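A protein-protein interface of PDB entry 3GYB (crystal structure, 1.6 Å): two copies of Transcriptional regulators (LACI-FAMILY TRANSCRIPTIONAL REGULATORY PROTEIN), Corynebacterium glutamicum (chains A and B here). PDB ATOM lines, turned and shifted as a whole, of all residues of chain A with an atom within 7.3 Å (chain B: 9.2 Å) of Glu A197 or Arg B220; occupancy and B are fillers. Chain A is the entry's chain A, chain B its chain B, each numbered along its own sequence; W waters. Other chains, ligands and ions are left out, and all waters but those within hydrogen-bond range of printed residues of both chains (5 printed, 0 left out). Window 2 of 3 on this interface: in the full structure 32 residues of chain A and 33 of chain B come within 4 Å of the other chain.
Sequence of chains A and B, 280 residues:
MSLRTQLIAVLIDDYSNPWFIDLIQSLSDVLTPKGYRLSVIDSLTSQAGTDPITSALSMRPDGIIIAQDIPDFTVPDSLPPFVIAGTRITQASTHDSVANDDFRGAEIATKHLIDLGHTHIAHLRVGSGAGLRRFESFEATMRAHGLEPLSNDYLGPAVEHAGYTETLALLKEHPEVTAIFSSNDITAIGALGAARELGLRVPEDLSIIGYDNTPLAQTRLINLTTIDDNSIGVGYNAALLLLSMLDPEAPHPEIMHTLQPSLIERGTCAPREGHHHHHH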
ATOM      1  N   GLU A 160      -4.589  -4.609  32.399  1.00  0.00           N
ATOM      2  CA  GLU A 160      -3.820  -5.721  31.866  1.00  0.00           C
ATOM      3  C   GLU A 160      -3.195  -6.601  32.934  1.00  0.00           C
ATOM      4  O   GLU A 160      -3.261  -7.821  32.845  1.00  0.00           O
ATOM      5  CB  GLU A 160      -2.727  -5.202  30.920  1.00  0.00           C
ATOM      6  CG  GLU A 160      -1.854  -6.279  30.267  1.00  0.00           C
ATOM      7  CD  GLU A 160      -0.777  -6.834  31.186  1.00  0.00           C
ATOM      8  OE1 GLU A 160      -0.270  -6.080  32.045  1.00  0.00           O
ATOM      9  OE2 GLU A 160      -0.416  -8.021  31.032  1.00  0.00           O
ATOM     10  N   TYR A 164      -3.625 -10.718  33.542  1.00  0.00           N
ATOM     11  CA  TYR A 164      -2.500 -11.629  33.562  1.00  0.00           C
ATOM     12  C   TYR A 164      -2.548 -12.547  34.781  1.00  0.00           C
ATOM     13  O   TYR A 164      -2.582 -13.763  34.637  1.00  0.00           O
ATOM     14  CB  TYR A 164      -1.187 -10.835  33.554  1.00  0.00           C
ATOM     15  CG  TYR A 164       0.050 -11.699  33.632  1.00  0.00           C
ATOM     16  CD1 TYR A 164       0.352 -12.612  32.621  1.00  0.00           C
ATOM     17  CD2 TYR A 164       0.927 -11.594  34.709  1.00  0.00           C
ATOM     18  CE1 TYR A 164       1.498 -13.401  32.683  1.00  0.00           C
ATOM     19  CE2 TYR A 164       2.085 -12.379  34.778  1.00  0.00           C
ATOM     20  CZ  TYR A 164       2.360 -13.278  33.760  1.00  0.00           C
ATOM     21  OH  TYR A 164       3.504 -14.048  33.814  1.00  0.00           O
ATOM     22  N   LEU A 168      -3.626 -16.626  35.061  1.00  0.00           N
ATOM     23  CA  LEU A 168      -2.707 -17.630  35.577  1.00  0.00           C
ATOM     24  C   LEU A 168      -3.364 -18.390  36.728  1.00  0.00           C
ATOM     25  O   LEU A 168      -3.192 -19.601  36.857  1.00  0.00           O
ATOM     26  CB  LEU A 168      -1.408 -16.983  36.063  1.00  0.00           C
ATOM     27  CG  LEU A 168      -0.442 -16.496  34.982  1.00  0.00           C
ATOM     28  CD1 LEU A 168       0.755 -15.828  35.654  1.00  0.00           C
ATOM     29  CD2 LEU A 168       0.017 -17.666  34.116  1.00  0.00           C
ATOM     30  N   ILE A 189      -5.337  -9.005  26.844  1.00  0.00           N
ATOM     31  CA  ILE A 189      -3.901  -8.867  26.620  1.00  0.00           C
ATOM     32  C   ILE A 189      -3.198  -9.585  27.767  1.00  0.00           C
ATOM     33  O   ILE A 189      -2.181 -10.248  27.568  1.00  0.00           O
ATOM     34  CB  ILE A 189      -3.461  -7.382  26.597  1.00  0.00           C
ATOM     35  CG1 ILE A 189      -4.178  -6.640  25.469  1.00  0.00           C
ATOM     36  CG2 ILE A 189      -1.953  -7.287  26.415  1.00  0.00           C
ATOM     37  CD1 ILE A 189      -4.017  -7.284  24.119  1.00  0.00           C
ATOM     38  N   GLY A 190      -3.753  -9.447  28.970  1.00  0.00           N
ATOM     39  CA  GLY A 190      -3.188 -10.122  30.125  1.00  0.00           C
ATOM     40  C   GLY A 190      -3.343 -11.626  29.984  1.00  0.00           C
ATOM     41  O   GLY A 190      -2.426 -12.397  30.296  1.00  0.00           O
ATOM     42  N   ALA A 191      -4.505 -12.053  29.504  1.00  0.00           N
ATOM     43  CA  ALA A 191      -4.764 -13.475  29.312  1.00  0.00           C
ATOM     44  C   ALA A 191      -3.791 -14.064  28.296  1.00  0.00           C
ATOM     45  O   ALA A 191      -3.304 -15.182  28.469  1.00  0.00           O
ATOM     46  CB  ALA A 191      -6.202 -13.690  28.847  1.00  0.00           C
ATOM     47  N   LEU A 192      -3.510 -13.314  27.230  1.00  0.00           N
ATOM     48  CA  LEU A 192      -2.576 -13.784  26.210  1.00  0.00           C
ATOM     49  C   LEU A 192      -1.177 -13.914  26.806  1.00  0.00           C
ATOM     50  O   LEU A 192      -0.429 -14.824  26.459  1.00  0.00           O
ATOM     51  CB  LEU A 192      -2.547 -12.817  25.020  1.00  0.00           C
ATOM     52  CG  LEU A 192      -3.792 -12.838  24.131  1.00  0.00           C
ATOM     53  CD1 LEU A 192      -3.811 -11.616  23.216  1.00  0.00           C
ATOM     54  CD2 LEU A 192      -3.818 -14.132  23.317  1.00  0.00           C
ATOM     55  N   GLY A 193      -0.827 -12.998  27.701  1.00  0.00           N
ATOM     56  CA  GLY A 193       0.478 -13.057  28.337  1.00  0.00           C
ATOM     57  C   GLY A 193       0.559 -14.274  29.243  1.00  0.00           C
ATOM     58  O   GLY A 193       1.593 -14.934  29.330  1.00  0.00           O
ATOM     59  N   ALA A 194      -0.539 -14.575  29.928  1.00  0.00           N
ATOM     60  CA  ALA A 194      -0.573 -15.730  30.819  1.00  0.00           C
ATOM     61  C   ALA A 194      -0.372 -17.002  30.003  1.00  0.00           C
ATOM     62  O   ALA A 194       0.393 -17.884  30.396  1.00  0.00           O
ATOM     63  CB  ALA A 194      -1.911 -15.778  31.572  1.00  0.00           C
ATOM     64  N   ALA A 195      -1.048 -17.091  28.859  1.00  0.00           N
ATOM     65  CA  ALA A 195      -0.911 -18.253  27.994  1.00  0.00           C
ATOM     66  C   ALA A 195       0.554 -18.406  27.579  1.00  0.00           C
ATOM     67  O   ALA A 195       1.109 -19.512  27.593  1.00  0.00           O
ATOM     68  CB  ALA A 195      -1.803 -18.098  26.763  1.00  0.00           C
ATOM     69  N   ARG A 196       1.186 -17.294  27.221  1.00  0.00           N
ATOM     70  CA  ARG A 196       2.587 -17.331  26.819  1.00  0.00           C
ATOM     71  C   ARG A 196       3.468 -17.825  27.976  1.00  0.00           C
ATOM     72  O   ARG A 196       4.343 -18.664  27.785  1.00  0.00           O
ATOM     73  CB  ARG A 196       3.048 -15.945  26.358  1.00  0.00           C
ATOM     74  CG  ARG A 196       4.452 -15.945  25.767  1.00  0.00           C
ATOM     75  CD  ARG A 196       4.917 -14.571  25.300  1.00  0.00           C
ATOM     76  NE  ARG A 196       6.232 -14.679  24.670  1.00  0.00           N
ATOM     77  CZ  ARG A 196       6.944 -13.659  24.199  1.00  0.00           C
ATOM     78  NH1 ARG A 196       6.482 -12.418  24.278  1.00  0.00           N
ATOM     79  NH2 ARG A 196       8.122 -13.889  23.634  1.00  0.00           N
ATOM     80  N   GLU A 197       3.229 -17.304  29.175  1.00  0.00           N
ATOM     81  CA  GLU A 197       3.996 -17.704  30.352  1.00  0.00           C
ATOM     82  C   GLU A 197       3.816 -19.194  30.642  1.00  0.00           C
ATOM     83  O   GLU A 197       4.744 -19.867  31.096  1.00  0.00           O
ATOM     84  CB  GLU A 197       3.551 -16.882  31.567  1.00  0.00           C
ATOM     85  CG  GLU A 197       4.213 -17.277  32.884  1.00  0.00           C
ATOM     86  CD  GLU A 197       5.729 -17.232  32.824  1.00  0.00           C
ATOM     87  OE1 GLU A 197       6.278 -16.296  32.206  1.00  0.00           O
ATOM     88  OE2 GLU A 197       6.371 -18.132  33.413  1.00  0.00           O
ATOM     89  N   LEU A 198       2.621 -19.706  30.367  1.00  0.00           N
ATOM     90  CA  LEU A 198       2.308 -21.110  30.608  1.00  0.00           C
ATOM     91  C   LEU A 198       2.756 -22.048  29.491  1.00  0.00           C
ATOM     92  O   LEU A 198       2.679 -23.267  29.633  1.00  0.00           O
ATOM     93  CB  LEU A 198       0.803 -21.270  30.835  1.00  0.00           C
ATOM     94  CG  LEU A 198       0.289 -20.757  32.181  1.00  0.00           C
ATOM     95  CD1 LEU A 198      -1.232 -20.714  32.178  1.00  0.00           C
ATOM     96  CD2 LEU A 198       0.812 -21.663  33.292  1.00  0.00           C
ATOM     97  N   GLY A 199       3.222 -21.483  28.386  1.00  0.00           N
ATOM     98  CA  GLY A 199       3.662 -22.309  27.274  1.00  0.00           C
ATOM     99  C   GLY A 199       2.488 -22.849  26.474  1.00  0.00           C
ATOM    100  O   GLY A 199       2.605 -23.854  25.770  1.00  0.00           O
ATOM    101  N   LEU A 200       1.340 -22.191  26.594  1.00  0.00           N
ATOM    102  CA  LEU A 200       0.153 -22.604  25.863  1.00  0.00           C
ATOM    103  C   LEU A 200       0.076 -21.823  24.562  1.00  0.00           C
ATOM    104  O   LEU A 200       0.157 -20.594  24.565  1.00  0.00           O
ATOM    105  CB  LEU A 200      -1.108 -22.323  26.681  1.00  0.00           C
ATOM    106  CG  LEU A 200      -1.271 -23.070  28.007  1.00  0.00           C
ATOM    107  CD1 LEU A 200      -2.438 -22.468  28.781  1.00  0.00           C
ATOM    108  CD2 LEU A 200      -1.504 -24.551  27.743  1.00  0.00           C
ATOM    109  N   VAL B 202      11.721 -13.876  17.979  1.00  0.00           N
ATOM    110  CA  VAL B 202      12.307 -12.760  18.701  1.00  0.00           C
ATOM    111  C   VAL B 202      12.499 -13.294  20.111  1.00  0.00           C
ATOM    112  O   VAL B 202      11.539 -13.714  20.754  1.00  0.00           O
ATOM    113  CB  VAL B 202      11.374 -11.526  18.719  1.00  0.00           C
ATOM    114  CG1 VAL B 202      11.979 -10.430  19.590  1.00  0.00           C
ATOM    115  CG2 VAL B 202      11.191 -11.003  17.298  1.00  0.00           C
ATOM    116  N   PRO B 215       3.525   1.264  28.995  1.00  0.00           N
ATOM    117  CA  PRO B 215       2.888   0.178  29.744  1.00  0.00           C
ATOM    118  C   PRO B 215       2.845  -1.083  28.878  1.00  0.00           C
ATOM    119  O   PRO B 215       2.936  -2.201  29.380  1.00  0.00           O
ATOM    120  CB  PRO B 215       1.497   0.737  30.029  1.00  0.00           C
ATOM    121  CG  PRO B 215       1.781   2.192  30.235  1.00  0.00           C
ATOM    122  CD  PRO B 215       2.730   2.502  29.085  1.00  0.00           C
ATOM    123  N   LEU B 216       2.709  -0.891  27.570  1.00  0.00           N
ATOM    124  CA  LEU B 216       2.671  -2.005  26.628  1.00  0.00           C
ATOM    125  C   LEU B 216       3.957  -2.826  26.677  1.00  0.00           C
ATOM    126  O   LEU B 216       3.927  -4.055  26.655  1.00  0.00           O
ATOM    127  CB  LEU B 216       2.475  -1.483  25.203  1.00  0.00           C
ATOM    128  CG  LEU B 216       1.187  -0.723  24.892  1.00  0.00           C
ATOM    129  CD1 LEU B 216       1.286  -0.096  23.499  1.00  0.00           C
ATOM    130  CD2 LEU B 216       0.002  -1.675  24.977  1.00  0.00           C
ATOM    131  N   ALA B 217       5.091  -2.135  26.727  1.00  0.00           N
ATOM    132  CA  ALA B 217       6.387  -2.807  26.758  1.00  0.00           C
ATOM    133  C   ALA B 217       6.535  -3.631  28.031  1.00  0.00           C
ATOM    134  O   ALA B 217       7.239  -4.645  28.053  1.00  0.00           O
ATOM    135  CB  ALA B 217       7.507  -1.771  26.683  1.00  0.00           C
ATOM    136  N   GLN B 218       5.858  -3.171  29.080  1.00  0.00           N
ATOM    137  CA  GLN B 218       5.890  -3.801  30.397  1.00  0.00           C
ATOM    138  C   GLN B 218       5.057  -5.073  30.525  1.00  0.00           C
ATOM    139  O   GLN B 218       5.222  -5.821  31.482  1.00  0.00           O
ATOM    140  CB  GLN B 218       5.407  -2.800  31.445  1.00  0.00           C
ATOM    141  CG  GLN B 218       6.273  -1.564  31.580  1.00  0.00           C
ATOM    142  CD  GLN B 218       5.615  -0.496  32.430  1.00  0.00           C
ATOM    143  OE1 GLN B 218       4.978  -0.797  33.442  1.00  0.00           O
ATOM    144  NE2 GLN B 218       5.768   0.761  32.027  1.00  0.00           N
ATOM    145  N   THR B 219       4.162  -5.319  29.577  1.00  0.00           N
ATOM    146  CA  THR B 219       3.313  -6.509  29.652  1.00  0.00           C
ATOM    147  C   THR B 219       4.089  -7.807  29.453  1.00  0.00           C
ATOM    148  O   THR B 219       5.141  -7.832  28.811  1.00  0.00           O
ATOM    149  CB  THR B 219       2.175  -6.461  28.607  1.00  0.00           C
ATOM    150  OG1 THR B 219       2.729  -6.495  27.282  1.00  0.00           O
ATOM    151  CG2 THR B 219       1.346  -5.197  28.783  1.00  0.00           C
ATOM    152  N   ARG B 220       3.580  -8.898  30.014  1.00  0.00           N
ATOM    153  CA  ARG B 220       4.254 -10.179  29.839  1.00  0.00           C
ATOM    154  C   ARG B 220       4.174 -10.611  28.375  1.00  0.00           C
ATOM    155  O   ARG B 220       5.105 -11.221  27.844  1.00  0.00           O
ATOM    156  CB  ARG B 220       3.607 -11.251  30.721  1.00  0.00           C
ATOM    157  CG  ARG B 220       4.122 -12.662  30.450  1.00  0.00           C
ATOM    158  CD  ARG B 220       5.565 -12.834  30.897  1.00  0.00           C
ATOM    159  NE  ARG B 220       6.122 -14.137  30.526  1.00  0.00           N
ATOM    160  CZ  ARG B 220       6.638 -14.429  29.333  1.00  0.00           C
ATOM    161  NH1 ARG B 220       6.676 -13.514  28.370  1.00  0.00           N
ATOM    162  NH2 ARG B 220       7.140 -15.637  29.107  1.00  0.00           N
ATOM    163  N   LEU B 221       3.062 -10.287  27.724  1.00  0.00           N
ATOM    164  CA  LEU B 221       2.860 -10.659  26.326  1.00  0.00           C
ATOM    165  C   LEU B 221       3.886 -10.035  25.391  1.00  0.00           C
ATOM    166  O   LEU B 221       4.471 -10.717  24.548  1.00  0.00           O
ATOM    167  CB  LEU B 221       1.459 -10.244  25.860  1.00  0.00           C
ATOM    168  CG  LEU B 221       1.140 -10.596  24.403  1.00  0.00           C
ATOM    169  CD1 LEU B 221       1.182 -12.108  24.242  1.00  0.00           C
ATOM    170  CD2 LEU B 221      -0.238 -10.049  24.012  1.00  0.00           C
ATOM    171  N   ILE B 222       4.098  -8.733  25.536  1.00  0.00           N
ATOM    172  CA  ILE B 222       5.039  -8.027  24.675  1.00  0.00           C
ATOM    173  C   ILE B 222       6.456  -8.127  25.247  1.00  0.00           C
ATOM    174  O   ILE B 222       7.407  -8.443  24.519  1.00  0.00           O
ATOM    175  CB  ILE B 222       4.576  -6.567  24.492  1.00  0.00           C
ATOM    176  CG1 ILE B 222       3.185  -6.569  23.836  1.00  0.00           C
ATOM    177  CG2 ILE B 222       5.563  -5.798  23.622  1.00  0.00           C
ATOM    178  CD1 ILE B 222       2.546  -5.201  23.705  1.00  0.00           C
ATOM    179  N   ASN B 223       6.593  -7.869  26.548  1.00  0.00           N
ATOM    180  CA  ASN B 223       7.880  -8.008  27.237  1.00  0.00           C
ATOM    181  C   ASN B 223       9.042  -7.442  26.411  1.00  0.00           C
ATOM    182  O   ASN B 223      10.033  -8.125  26.135  1.00  0.00           O
ATOM    183  CB  ASN B 223       8.082  -9.500  27.525  1.00  0.00           C
ATOM    184  CG  ASN B 223       9.166  -9.758  28.537  1.00  0.00           C
ATOM    185  OD1 ASN B 223       9.282  -9.043  29.527  1.00  0.00           O
ATOM    186  ND2 ASN B 223       9.956 -10.798  28.306  1.00  0.00           N
ATOM    187  N   LEU B 224       8.916  -6.169  26.064  1.00  0.00           N
ATOM    188  CA  LEU B 224       9.881  -5.477  25.213  1.00  0.00           C
ATOM    189  C   LEU B 224      11.068  -4.790  25.876  1.00  0.00           C
ATOM    190  O   LEU B 224      10.902  -3.997  26.800  1.00  0.00           O
ATOM    191  CB  LEU B 224       9.119  -4.446  24.379  1.00  0.00           C
ATOM    192  CG  LEU B 224       9.888  -3.426  23.539  1.00  0.00           C
ATOM    193  CD1 LEU B 224      10.550  -4.111  22.350  1.00  0.00           C
ATOM    194  CD2 LEU B 224       8.909  -2.354  23.073  1.00  0.00           C
ATOM    195  N   ARG B 266      14.437  -6.789  28.768  1.00  0.00           N
ATOM    196  CA  ARG B 266      13.340  -7.729  28.917  1.00  0.00           C
ATOM    197  C   ARG B 266      13.631  -8.919  28.009  1.00  0.00           C
ATOM    198  O   ARG B 266      14.758  -9.413  28.000  1.00  0.00           O
ATOM    199  CB  ARG B 266      11.988  -7.066  28.607  1.00  0.00           C
ATOM    200  CG  ARG B 266      11.614  -5.999  29.646  1.00  0.00           C
ATOM    201  CD  ARG B 266      10.115  -5.691  29.711  1.00  0.00           C
ATOM    202  NE  ARG B 266       9.825  -4.748  30.793  1.00  0.00           N
ATOM    203  CZ  ARG B 266       9.799  -3.424  30.663  1.00  0.00           C
ATOM    204  NH1 ARG B 266      10.031  -2.862  29.481  1.00  0.00           N
ATOM    205  NH2 ARG B 266       9.578  -2.653  31.724  1.00  0.00           N
ATOM    206  N   GLY B 267      12.664  -9.370  27.220  1.00  0.00           N
ATOM    207  CA  GLY B 267      12.932 -10.542  26.401  1.00  0.00           C
ATOM    208  C   GLY B 267      13.053 -10.430  24.893  1.00  0.00           C
ATOM    209  O   GLY B 267      12.989 -11.452  24.212  1.00  0.00           O
ATOM    210  N   THR B 268      13.261  -9.228  24.361  1.00  0.00           N
ATOM    211  CA  THR B 268      13.344  -9.073  22.908  1.00  0.00           C
ATOM    212  C   THR B 268      14.734  -8.937  22.289  1.00  0.00           C
ATOM    213  O   THR B 268      14.858  -8.746  21.074  1.00  0.00           O
ATOM    214  CB  THR B 268      12.476  -7.889  22.441  1.00  0.00           C
ATOM    215  OG1 THR B 268      12.865  -6.704  23.139  1.00  0.00           O
ATOM    216  CG2 THR B 268      11.010  -8.170  22.723  1.00  0.00           C
HETATM  217  O   HOH W   1       8.525 -15.709  26.605  1.00  0.00           O
HETATM  218  O   HOH W   2       9.426 -11.062  24.746  1.00  0.00           O
HETATM  219  O   HOH W   3       9.865 -11.887  22.206  1.00  0.00           O
HETATM  220  O   HOH W   4       0.353  -9.606  28.898  1.00  0.00           O
HETATM  221  O   HOH W   5      10.864 -15.146  23.093  1.00  0.00           O
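Water W4 lies within hydrogen-bond range of OE2 of Glu A160, O of Ile A189, N of Leu B221 and N of Arg B220.
Water W5 lies within hydrogen-bond range of O of Val B202 (2.8 Å) and NH2 of Arg A196 (3.1 Å).
Water W1 bridges NH2 of Arg B220 (2.9 Å) and NE of Arg A196 (3.2 Å).
Water W3 lies within hydrogen-bond range of O of Val B202 and NH2 of Arg A196.
Water W2 lies within hydrogen-bond range of NH1 of Arg A196 (3.3 Å), O of Asn B223 (3.3 Å) and O of Ile B222 (3.3 Å).
Of chain B, only Arg B220 (2.7 Å) comes within 4 Å of Glu A197.
Printed residues of chain A within 4 Å of Arg B220: Tyr A164, Gly A193, Arg A196 and Glu A197.
Of the printed residues of chain B, Tyr A164 touches Arg B220.
Of the printed residues of chain B, Glu A160 touches Thr B219.
Printed residues of chain A within 4 Å of Thr B219: Glu A160 (3.6 Å).
Of the printed residues of chain A, Leu B221 touches Leu A192 (3.7 Å), Gly A193 (3.8 Å) and Arg A196 (2.6 Å).
Of the printed residues of chain B, Leu A192 touches Leu B221 (3.7 Å).
Leu A200 touches none of the printed residues of chain B.
The nearest residue of chain B that does not touch Glu A197 is Leu B221 (7.2 Å).
Of the 15 printed residues of chain A, 6 touch a printed residue of chain B.
Along chain A the printed residues that touch a printed residue of chain B span positions 160 to 197.
Of the 14 printed residues of chain B, 3 touch a printed residue of chain A.
Printed residues of chain B that touch a printed residue of chain A: Thr B219, Arg B220 and Leu B221.
Hydrophobic or aromatic side chains of chain B within 4 Å of the printed part of chain A: Leu B221.
Among the printed residues, 8 pairs touch across the chains.
Among the printed residues, Asp or Glu carboxylates within 4 Å of a Lys or Arg side-chain nitrogen of the other chain: Glu A197 with Arg B220 (2.7 Å).
CG2 of Thr B219 touches CD of Glu A160, at 3.6 Å.
CG of Arg B220 touches CE1 of Tyr A164 (3.5 Å).
Leu A192 touches Leu B221.
Arg B220 touches Gly A193 (CG to O, 3.6 Å).
Gly A193 touches Leu B221 (CA to N, 3.8 Å).
Arg B220 touches Arg A196 (NH1 to CD, 3.7 Å).
The guanidinium group of Arg A196 is in hydrogen-bond range of the backbone carbonyl oxygen of Leu B221 (2.6 Å).
The guanidinium group (NE) of Arg B220 is in salt-bridge range of the side-chain carboxylate (OE1) of Glu A197, at 2.7 Å.
O of Leu B216 sits at hydrogen-bond distance from OG1 of Thr B219 (2.8 Å).
The backbone NH (N) of Ile B222 lies within hydrogen-bond range of the side-chain hydroxyl (OG1) of Thr B219 (3.2 Å).
No position is printed for both chains.
Of the 8 pairs that touch across the chains among the printed residues, none has its exchanged pair printed and touching as well.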
